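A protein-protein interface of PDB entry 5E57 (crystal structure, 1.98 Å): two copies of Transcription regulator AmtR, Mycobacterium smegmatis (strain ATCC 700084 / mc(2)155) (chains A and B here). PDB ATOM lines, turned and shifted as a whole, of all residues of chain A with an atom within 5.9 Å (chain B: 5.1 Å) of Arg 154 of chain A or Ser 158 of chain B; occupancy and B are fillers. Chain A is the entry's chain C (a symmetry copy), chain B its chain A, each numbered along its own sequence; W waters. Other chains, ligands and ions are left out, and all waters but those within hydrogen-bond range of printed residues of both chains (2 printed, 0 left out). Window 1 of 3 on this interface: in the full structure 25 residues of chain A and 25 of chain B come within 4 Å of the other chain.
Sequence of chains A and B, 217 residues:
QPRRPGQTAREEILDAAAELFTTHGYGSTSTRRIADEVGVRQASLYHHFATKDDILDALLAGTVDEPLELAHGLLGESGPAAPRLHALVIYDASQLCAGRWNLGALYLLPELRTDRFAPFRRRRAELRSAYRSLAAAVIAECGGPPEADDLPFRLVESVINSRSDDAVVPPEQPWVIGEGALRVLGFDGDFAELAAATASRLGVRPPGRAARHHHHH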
ATOM      1  N   ARG A 124      22.688  11.445   1.495  1.00  0.00           N
ATOM      2  CA  ARG A 124      23.109  10.078   1.269  1.00  0.00           C
ATOM      3  C   ARG A 124      21.871   9.201   0.937  1.00  0.00           C
ATOM      4  O   ARG A 124      21.918   8.352   0.034  1.00  0.00           O
ATOM      5  CB  ARG A 124      23.884   9.536   2.485  1.00  0.00           C
ATOM      6  CG  ARG A 124      24.284   8.094   2.302  1.00  0.00           C
ATOM      7  CD  ARG A 124      25.279   7.533   3.333  1.00  0.00           C
ATOM      8  NE  ARG A 124      25.215   6.088   3.259  1.00  0.00           N
ATOM      9  CZ  ARG A 124      24.318   5.370   3.927  1.00  0.00           C
ATOM     10  NH1 ARG A 124      23.504   5.957   4.822  1.00  0.00           N
ATOM     11  NH2 ARG A 124      24.255   4.066   3.752  1.00  0.00           N
ATOM     12  N   ARG A 128      21.140   6.857  -2.394  1.00  0.00           N
ATOM     13  CA  ARG A 128      20.604   5.481  -2.282  1.00  0.00           C
ATOM     14  C   ARG A 128      19.338   5.317  -3.119  1.00  0.00           C
ATOM     15  O   ARG A 128      19.135   4.337  -3.833  1.00  0.00           O
ATOM     16  CB  ARG A 128      20.294   5.163  -0.840  1.00  0.00           C
ATOM     17  CG  ARG A 128      19.834   3.755  -0.614  1.00  0.00           C
ATOM     18  CD  ARG A 128      19.372   3.588   0.823  1.00  0.00           C
ATOM     19  NE  ARG A 128      18.811   2.259   1.018  1.00  0.00           N
ATOM     20  CZ  ARG A 128      18.086   1.906   2.055  1.00  0.00           C
ATOM     21  NH1 ARG A 128      17.882   2.742   3.029  1.00  0.00           N
ATOM     22  NH2 ARG A 128      17.621   0.685   2.156  1.00  0.00           N
ATOM     23  N   ASP A 150      18.139  -2.603  -3.924  1.00  0.00           N
ATOM     24  CA  ASP A 150      19.098  -1.944  -2.974  1.00  0.00           C
ATOM     25  C   ASP A 150      20.527  -2.450  -3.084  1.00  0.00           C
ATOM     26  O   ASP A 150      21.431  -1.802  -2.598  1.00  0.00           O
ATOM     27  CB  ASP A 150      18.638  -2.085  -1.517  1.00  0.00           C
ATOM     28  CG  ASP A 150      19.150  -0.977  -0.618  1.00  0.00           C
ATOM     29  OD1 ASP A 150      19.214   0.186  -1.055  1.00  0.00           O
ATOM     30  OD2 ASP A 150      19.482  -1.216   0.553  1.00  0.00           O
ATOM     31  N   LEU A 151      20.790  -3.562  -3.774  1.00  0.00           N
ATOM     32  CA  LEU A 151      22.053  -4.222  -3.570  1.00  0.00           C
ATOM     33  C   LEU A 151      23.221  -3.547  -4.290  1.00  0.00           C
ATOM     34  O   LEU A 151      24.354  -3.620  -3.823  1.00  0.00           O
ATOM     35  CB  LEU A 151      21.943  -5.707  -3.946  1.00  0.00           C
ATOM     36  CG  LEU A 151      20.991  -6.576  -3.143  1.00  0.00           C
ATOM     37  CD1 LEU A 151      21.197  -8.042  -3.573  1.00  0.00           C
ATOM     38  CD2 LEU A 151      21.217  -6.426  -1.653  1.00  0.00           C
ATOM     39  N   PRO A 152      22.969  -2.859  -5.407  1.00  0.00           N
ATOM     40  CA  PRO A 152      24.107  -2.222  -6.080  1.00  0.00           C
ATOM     41  C   PRO A 152      24.736  -1.145  -5.240  1.00  0.00           C
ATOM     42  O   PRO A 152      25.981  -1.030  -5.196  1.00  0.00           O
ATOM     43  CB  PRO A 152      23.498  -1.674  -7.364  1.00  0.00           C
ATOM     44  CG  PRO A 152      22.466  -2.705  -7.658  1.00  0.00           C
ATOM     45  CD  PRO A 152      21.858  -3.085  -6.329  1.00  0.00           C
ATOM     46  N   PHE A 153      23.877  -0.451  -4.496  1.00  0.00           N
ATOM     47  CA  PHE A 153      24.319   0.562  -3.572  1.00  0.00           C
ATOM     48  C   PHE A 153      25.145  -0.076  -2.467  1.00  0.00           C
ATOM     49  O   PHE A 153      26.176   0.470  -2.094  1.00  0.00           O
ATOM     50  CB  PHE A 153      23.121   1.253  -2.933  1.00  0.00           C
ATOM     51  CG  PHE A 153      23.477   2.266  -1.870  1.00  0.00           C
ATOM     52  CD1 PHE A 153      24.060   3.465  -2.214  1.00  0.00           C
ATOM     53  CD2 PHE A 153      23.073   2.090  -0.561  1.00  0.00           C
ATOM     54  CE1 PHE A 153      24.298   4.458  -1.244  1.00  0.00           C
ATOM     55  CE2 PHE A 153      23.338   3.038   0.419  1.00  0.00           C
ATOM     56  CZ  PHE A 153      23.944   4.228   0.081  1.00  0.00           C
ATOM     57  N   ARG A 154      24.650  -1.171  -1.910  1.00  0.00           N
ATOM     58  CA  ARG A 154      25.393  -1.865  -0.830  1.00  0.00           C
ATOM     59  C   ARG A 154      26.735  -2.414  -1.323  1.00  0.00           C
ATOM     60  O   ARG A 154      27.675  -2.428  -0.576  1.00  0.00           O
ATOM     61  CB  ARG A 154      24.568  -2.969  -0.286  1.00  0.00           C
ATOM     62  CG  ARG A 154      23.227  -2.523   0.229  1.00  0.00           C
ATOM     63  CD  ARG A 154      23.417  -1.438   1.296  1.00  0.00           C
ATOM     64  NE  ARG A 154      22.122  -0.959   1.782  1.00  0.00           N
ATOM     65  CZ  ARG A 154      21.996  -0.007   2.677  1.00  0.00           C
ATOM     66  NH1 ARG A 154      23.077   0.566   3.166  1.00  0.00           N
ATOM     67  NH2 ARG A 154      20.784   0.396   3.063  1.00  0.00           N
ATOM     68  N   LEU A 155      26.826  -2.827  -2.588  1.00  0.00           N
ATOM     69  CA  LEU A 155      28.089  -3.322  -3.167  1.00  0.00           C
ATOM     70  C   LEU A 155      29.119  -2.228  -3.304  1.00  0.00           C
ATOM     71  O   LEU A 155      30.292  -2.414  -2.998  1.00  0.00           O
ATOM     72  CB  LEU A 155      27.862  -4.048  -4.523  1.00  0.00           C
ATOM     73  CG  LEU A 155      27.303  -5.469  -4.338  1.00  0.00           C
ATOM     74  CD1 LEU A 155      26.524  -5.992  -5.539  1.00  0.00           C
ATOM     75  CD2 LEU A 155      28.401  -6.474  -3.976  1.00  0.00           C
ATOM     76  N   VAL A 156      28.663  -1.058  -3.721  1.00  0.00           N
ATOM     77  CA  VAL A 156      29.494   0.133  -3.847  1.00  0.00           C
ATOM     78  C   VAL A 156      30.006   0.514  -2.476  1.00  0.00           C
ATOM     79  O   VAL A 156      31.220   0.626  -2.330  1.00  0.00           O
ATOM     80  CB  VAL A 156      28.756   1.361  -4.472  1.00  0.00           C
ATOM     81  CG1 VAL A 156      29.540   2.679  -4.362  1.00  0.00           C
ATOM     82  CG2 VAL A 156      28.449   1.131  -5.920  1.00  0.00           C
ATOM     83  N   GLU A 157      29.131   0.592  -1.472  1.00  0.00           N
ATOM     84  CA  GLU A 157      29.555   0.981  -0.111  1.00  0.00           C
ATOM     85  C   GLU A 157      30.441  -0.079   0.537  1.00  0.00           C
ATOM     86  O   GLU A 157      31.148   0.230   1.451  1.00  0.00           O
ATOM     87  CB  GLU A 157      28.368   1.387   0.811  1.00  0.00           C
ATOM     88  CG  GLU A 157      27.872   2.792   0.400  1.00  0.00           C
ATOM     89  CD  GLU A 157      27.095   3.510   1.426  1.00  0.00           C
ATOM     90  OE1 GLU A 157      26.903   4.771   1.217  1.00  0.00           O
ATOM     91  OE2 GLU A 157      26.704   2.842   2.380  1.00  0.00           O
ATOM     92  N   SER A 158      30.437  -1.287   0.012  1.00  0.00           N
ATOM     93  CA  SER A 158      31.245  -2.404   0.565  1.00  0.00           C
ATOM     94  C   SER A 158      32.726  -2.136   0.405  1.00  0.00           C
ATOM     95  O   SER A 158      33.552  -2.732   1.147  1.00  0.00           O
ATOM     96  CB  SER A 158      30.842  -3.792  -0.007  1.00  0.00           C
ATOM     97  OG  SER A 158      31.394  -4.038  -1.305  1.00  0.00           O
ATOM     98  N   VAL A 159      33.097  -1.257  -0.519  1.00  0.00           N
ATOM     99  CA  VAL A 159      34.523  -0.943  -0.662  1.00  0.00           C
ATOM    100  C   VAL A 159      35.065  -0.311   0.602  1.00  0.00           C
ATOM    101  O   VAL A 159      36.283  -0.396   0.854  1.00  0.00           O
ATOM    102  CB  VAL A 159      34.904  -0.051  -1.889  1.00  0.00           C
ATOM    103  CG1 VAL A 159      34.430  -0.645  -3.206  1.00  0.00           C
ATOM    104  CG2 VAL A 159      34.456   1.385  -1.701  1.00  0.00           C
ATOM    105  N   PHE B 153      30.773 -12.407   1.058  1.00  0.00           N
ATOM    106  CA  PHE B 153      31.074 -11.890   2.426  1.00  0.00           C
ATOM    107  C   PHE B 153      30.635 -10.454   2.561  1.00  0.00           C
ATOM    108  O   PHE B 153      29.999 -10.088   3.543  1.00  0.00           O
ATOM    109  CB  PHE B 153      32.552 -12.047   2.743  1.00  0.00           C
ATOM    110  CG  PHE B 153      32.982 -11.473   4.053  1.00  0.00           C
ATOM    111  CD1 PHE B 153      32.659 -12.068   5.220  1.00  0.00           C
ATOM    112  CD2 PHE B 153      33.864 -10.374   4.091  1.00  0.00           C
ATOM    113  CE1 PHE B 153      33.130 -11.558   6.439  1.00  0.00           C
ATOM    114  CE2 PHE B 153      34.318  -9.866   5.284  1.00  0.00           C
ATOM    115  CZ  PHE B 153      33.951 -10.458   6.463  1.00  0.00           C
ATOM    116  N   ARG B 154      30.979  -9.651   1.615  1.00  0.00           N
ATOM    117  CA  ARG B 154      30.637  -8.226   1.679  1.00  0.00           C
ATOM    118  C   ARG B 154      29.118  -8.004   1.648  1.00  0.00           C
ATOM    119  O   ARG B 154      28.625  -7.162   2.381  1.00  0.00           O
ATOM    120  CB  ARG B 154      31.301  -7.485   0.558  1.00  0.00           C
ATOM    121  CG  ARG B 154      32.814  -7.573   0.539  1.00  0.00           C
ATOM    122  CD  ARG B 154      33.403  -6.979   1.793  1.00  0.00           C
ATOM    123  NE  ARG B 154      34.824  -7.264   1.942  1.00  0.00           N
ATOM    124  CZ  ARG B 154      35.526  -7.063   3.061  1.00  0.00           C
ATOM    125  NH1 ARG B 154      34.971  -6.605   4.147  1.00  0.00           N
ATOM    126  NH2 ARG B 154      36.800  -7.379   3.108  1.00  0.00           N
ATOM    127  N   LEU B 155      28.389  -8.791   0.864  1.00  0.00           N
ATOM    128  CA  LEU B 155      26.912  -8.754   0.835  1.00  0.00           C
ATOM    129  C   LEU B 155      26.297  -9.119   2.141  1.00  0.00           C
ATOM    130  O   LEU B 155      25.374  -8.446   2.622  1.00  0.00           O
ATOM    131  CB  LEU B 155      26.319  -9.630  -0.272  1.00  0.00           C
ATOM    132  CG  LEU B 155      26.482  -8.979  -1.625  1.00  0.00           C
ATOM    133  CD1 LEU B 155      26.388  -9.991  -2.745  1.00  0.00           C
ATOM    134  CD2 LEU B 155      25.430  -7.905  -1.783  1.00  0.00           C
ATOM    135  N   VAL B 156      26.880 -10.087   2.831  1.00  0.00           N
ATOM    136  CA  VAL B 156      26.358 -10.433   4.163  1.00  0.00           C
ATOM    137  C   VAL B 156      26.558  -9.341   5.178  1.00  0.00           C
ATOM    138  O   VAL B 156      25.611  -9.000   5.978  1.00  0.00           O
ATOM    139  CB  VAL B 156      27.024 -11.721   4.697  1.00  0.00           C
ATOM    140  CG1 VAL B 156      26.751 -11.945   6.163  1.00  0.00           C
ATOM    141  CG2 VAL B 156      26.635 -12.905   3.850  1.00  0.00           C
ATOM    142  N   GLU B 157      27.759  -8.762   5.165  1.00  0.00           N
ATOM    143  CA  GLU B 157      28.080  -7.666   6.067  1.00  0.00           C
ATOM    144  C   GLU B 157      27.297  -6.398   5.720  1.00  0.00           C
ATOM    145  O   GLU B 157      27.083  -5.552   6.585  1.00  0.00           O
ATOM    146  CB  GLU B 157      29.634  -7.420   6.143  1.00  0.00           C
ATOM    147  CG  GLU B 157      30.303  -8.597   6.923  1.00  0.00           C
ATOM    148  CD  GLU B 157      31.568  -8.220   7.652  1.00  0.00           C
ATOM    149  OE1 GLU B 157      32.183  -7.221   7.230  1.00  0.00           O
ATOM    150  OE2 GLU B 157      31.974  -8.964   8.616  1.00  0.00           O
ATOM    151  N   SER B 158      26.803  -6.293   4.494  1.00  0.00           N
ATOM    152  CA  SER B 158      25.994  -5.127   4.149  1.00  0.00           C
ATOM    153  C   SER B 158      24.733  -5.014   4.967  1.00  0.00           C
ATOM    154  O   SER B 158      24.134  -3.930   5.092  1.00  0.00           O
ATOM    155  CB  SER B 158      25.687  -5.056   2.662  1.00  0.00           C
ATOM    156  OG  SER B 158      24.592  -5.835   2.334  1.00  0.00           O
ATOM    157  N   VAL B 159      24.307  -6.075   5.600  1.00  0.00           N
ATOM    158  CA  VAL B 159      23.061  -5.941   6.427  1.00  0.00           C
ATOM    159  C   VAL B 159      23.251  -4.942   7.602  1.00  0.00           C
ATOM    160  O   VAL B 159      22.282  -4.329   8.087  1.00  0.00           O
ATOM    161  CB  VAL B 159      22.456  -7.305   6.844  1.00  0.00           C
ATOM    162  CG1 VAL B 159      22.380  -8.250   5.668  1.00  0.00           C
ATOM    163  CG2 VAL B 159      23.219  -7.959   7.984  1.00  0.00           C
ATOM    164  N   ILE B 160      24.503  -4.823   8.038  1.00  0.00           N
ATOM    165  CA  ILE B 160      24.902  -3.896   9.083  1.00  0.00           C
ATOM    166  C   ILE B 160      24.609  -2.455   8.611  1.00  0.00           C
ATOM    167  O   ILE B 160      23.958  -1.698   9.329  1.00  0.00           O
ATOM    168  CB  ILE B 160      26.373  -3.998   9.442  1.00  0.00           C
ATOM    169  CG1 ILE B 160      26.758  -5.328  10.092  1.00  0.00           C
ATOM    170  CG2 ILE B 160      26.767  -2.860  10.399  1.00  0.00           C
ATOM    171  CD1 ILE B 160      28.242  -5.669   9.834  1.00  0.00           C
ATOM    172  N   ASN B 161      25.003  -2.145   7.400  1.00  0.00           N
ATOM    173  CA  ASN B 161      24.674  -0.859   6.799  1.00  0.00           C
ATOM    174  C   ASN B 161      23.154  -0.674   6.614  1.00  0.00           C
ATOM    175  O   ASN B 161      22.647   0.415   6.817  1.00  0.00           O
ATOM    176  CB  ASN B 161      25.368  -0.710   5.466  1.00  0.00           C
ATOM    177  CG  ASN B 161      26.882  -0.898   5.570  1.00  0.00           C
ATOM    178  OD1 ASN B 161      27.647   0.059   5.494  1.00  0.00           O
ATOM    179  ND2 ASN B 161      27.316  -2.147   5.754  1.00  0.00           N
ATOM    180  N   SER B 162      22.421  -1.723   6.231  1.00  0.00           N
ATOM    181  CA  SER B 162      20.940  -1.645   6.093  1.00  0.00           C
ATOM    182  C   SER B 162      20.270  -1.312   7.419  1.00  0.00           C
ATOM    183  O   SER B 162      19.378  -0.468   7.471  1.00  0.00           O
ATOM    184  CB  SER B 162      20.328  -2.937   5.546  1.00  0.00           C
ATOM    185  OG  SER B 162      20.829  -3.252   4.262  1.00  0.00           O
ATOM    186  N   ASP B 165      20.722   2.345   8.232  1.00  0.00           N
ATOM    187  CA  ASP B 165      19.887   3.229   7.405  1.00  0.00           C
ATOM    188  C   ASP B 165      18.390   3.093   7.753  1.00  0.00           C
ATOM    189  O   ASP B 165      17.665   4.085   7.731  1.00  0.00           O
ATOM    190  CB  ASP B 165      20.090   2.903   5.933  1.00  0.00           C
ATOM    191  CG  ASP B 165      21.464   3.291   5.419  1.00  0.00           C
ATOM    192  OD1 ASP B 165      22.073   4.108   6.068  1.00  0.00           O
ATOM    193  OD2 ASP B 165      21.910   2.886   4.308  1.00  0.00           O
ATOM    194  N   ASP B 166      17.938   1.882   8.062  1.00  0.00           N
ATOM    195  CA  ASP B 166      16.522   1.563   8.185  1.00  0.00           C
ATOM    196  C   ASP B 166      16.007   1.138   9.549  1.00  0.00           C
ATOM    197  O   ASP B 166      16.619   0.368  10.291  1.00  0.00           O
ATOM    198  CB  ASP B 166      16.219   0.456   7.227  1.00  0.00           C
ATOM    199  CG  ASP B 166      16.322   0.903   5.851  1.00  0.00           C
ATOM    200  OD1 ASP B 166      16.269   2.122   5.681  1.00  0.00           O
ATOM    201  OD2 ASP B 166      16.539   0.091   4.947  1.00  0.00           O
ATOM    202  N   ILE B 177      19.806 -11.311   0.205  1.00  0.00           N
ATOM    203  CA  ILE B 177      21.234 -11.339   0.233  1.00  0.00           C
ATOM    204  C   ILE B 177      21.784 -12.691  -0.303  1.00  0.00           C
ATOM    205  O   ILE B 177      22.768 -12.708  -1.009  1.00  0.00           O
ATOM    206  CB  ILE B 177      21.715 -11.118   1.684  1.00  0.00           C
ATOM    207  CG1 ILE B 177      21.416  -9.666   2.081  1.00  0.00           C
ATOM    208  CG2 ILE B 177      23.195 -11.464   1.842  1.00  0.00           C
ATOM    209  CD1 ILE B 177      22.352  -8.689   1.453  1.00  0.00           C
HETATM  210  O   HOH W   1      27.194   2.961   5.159  1.00  0.00           O
HETATM  211  O   HOH W   2      25.822   0.270   2.552  1.00  0.00           O
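OD1 of Asp 165 of chain B is in salt-bridge range of NH1 of Arg 124 of chain A (2.6 Å).
The side-chain carboxylate of Asp 165 of chain B lies within salt-bridge range of the guanidinium group of Arg 154 of chain A, 2.8 Å away.
The guanidinium group of Arg 128 of chain A lies within salt-bridge range of the side-chain carboxylate of Asp 166 of chain B (3.1 Å).
The backbone carbonyl oxygen (O) of Leu 155 of chain B is in hydrogen-bond range of the side-chain hydroxyl (OG) of Ser 158 of chain B, 2.7 Å away.
The backbone carbonyl oxygen (O) of Ser 158 of chain B lies within hydrogen-bond range of the side-chain hydroxyl (OG) of Ser 162 of chain B, at 3.5 Å.
The guanidinium group (NE) of Arg 124 of chain A is in salt-bridge range of the side-chain carboxylate (OE1) of Glu 157 of chain A.
The guanidinium group (NE) of Arg 128 of chain A lies within salt-bridge range of the side-chain carboxylate (OD1) of Asp 150 of chain A (3.0 Å).
OD2 of Asp 150 of chain A is in salt-bridge range of NE of Arg 154 of chain A, at 2.9 Å.
O of Leu 155 of chain A lies within hydrogen-bond range of OG of Ser 158 of chain A, at 2.6 Å.
Among the printed residues, merely in contact across the chains: Arg 128 of chain A with Asp 165 of chain B, Arg 154 of chain A with Ser 158 of chain B, Arg 154 of chain A with Asn 161 of chain B, Arg 154 of chain A with Ser 162 of chain B, Leu 155 of chain A with Leu 155 of chain B and Ser 158 of chain A with Arg 154 of chain B.
Arg 154 of chain A touches four residues of chain B.
Of the printed residues of chain B, Arg 128 of chain A touches Asp 165 (3.7 Å) and Asp 166 (3.1 Å).
Printed residues of chain A within 4 Å of Leu 155 of chain B: Leu 155 (3.9 Å).
Printed residues of chain B within 4 Å of Arg 124 of chain A: Asp 165 (2.6 Å).
Of the printed residues of chain A, Asn 161 of chain B touches Arg 154 (3.5 Å).
Pro 152 of chain A touches none of the printed residues of chain B.
The nearest residue of chain A that does not touch Ser 158 of chain B is Leu 151 of chain A (5.3 Å).
Of the 12 printed residues of chain A, 5 touch a printed residue of chain B.
Printed residues of chain A that touch a printed residue of chain B: Arg 124, Arg 128, Arg 154, Leu 155 and Ser 158.
Hydrophobic or aromatic side chains of chain A within 4 Å of the printed part of chain B: Leu 155.
Along chain A the printed residues that touch a printed residue of chain B span positions 124 to 158.
Printed residues of chain B that touch a printed residue of chain A: Arg 154, Leu 155, Ser 158, Asn 161, Ser 162, Asp 165 and Asp 166.
Hydrophobic or aromatic side chains of chain B within 4 Å of the printed part of chain A: Leu 155.
Arg 154 of chain A touches Ser 158 of chain B, and with the chains exchanged Ser 158 of chain A touches Arg 154 of chain B.
Leu 155 of chain A touches its own counterpart, Leu 155 of chain B.
Positions printed for both chains: 153, 154, 155, 156, 157, 158 and 159.
Water W2 lies within hydrogen-bond range of OE2 of Glu 157 of chain A (2.7 Å), NH1 of Arg 154 of chain A (2.8 Å) and OD1 of Asn 161 of chain B (3.5 Å).
Water W1 lies within hydrogen-bond range of OE2 of Glu 157 of chain A (2.8 Å), OD1 of Asn 161 of chain B (3.0 Å) and NH2 of Arg 124 of chain A (3.4 Å).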
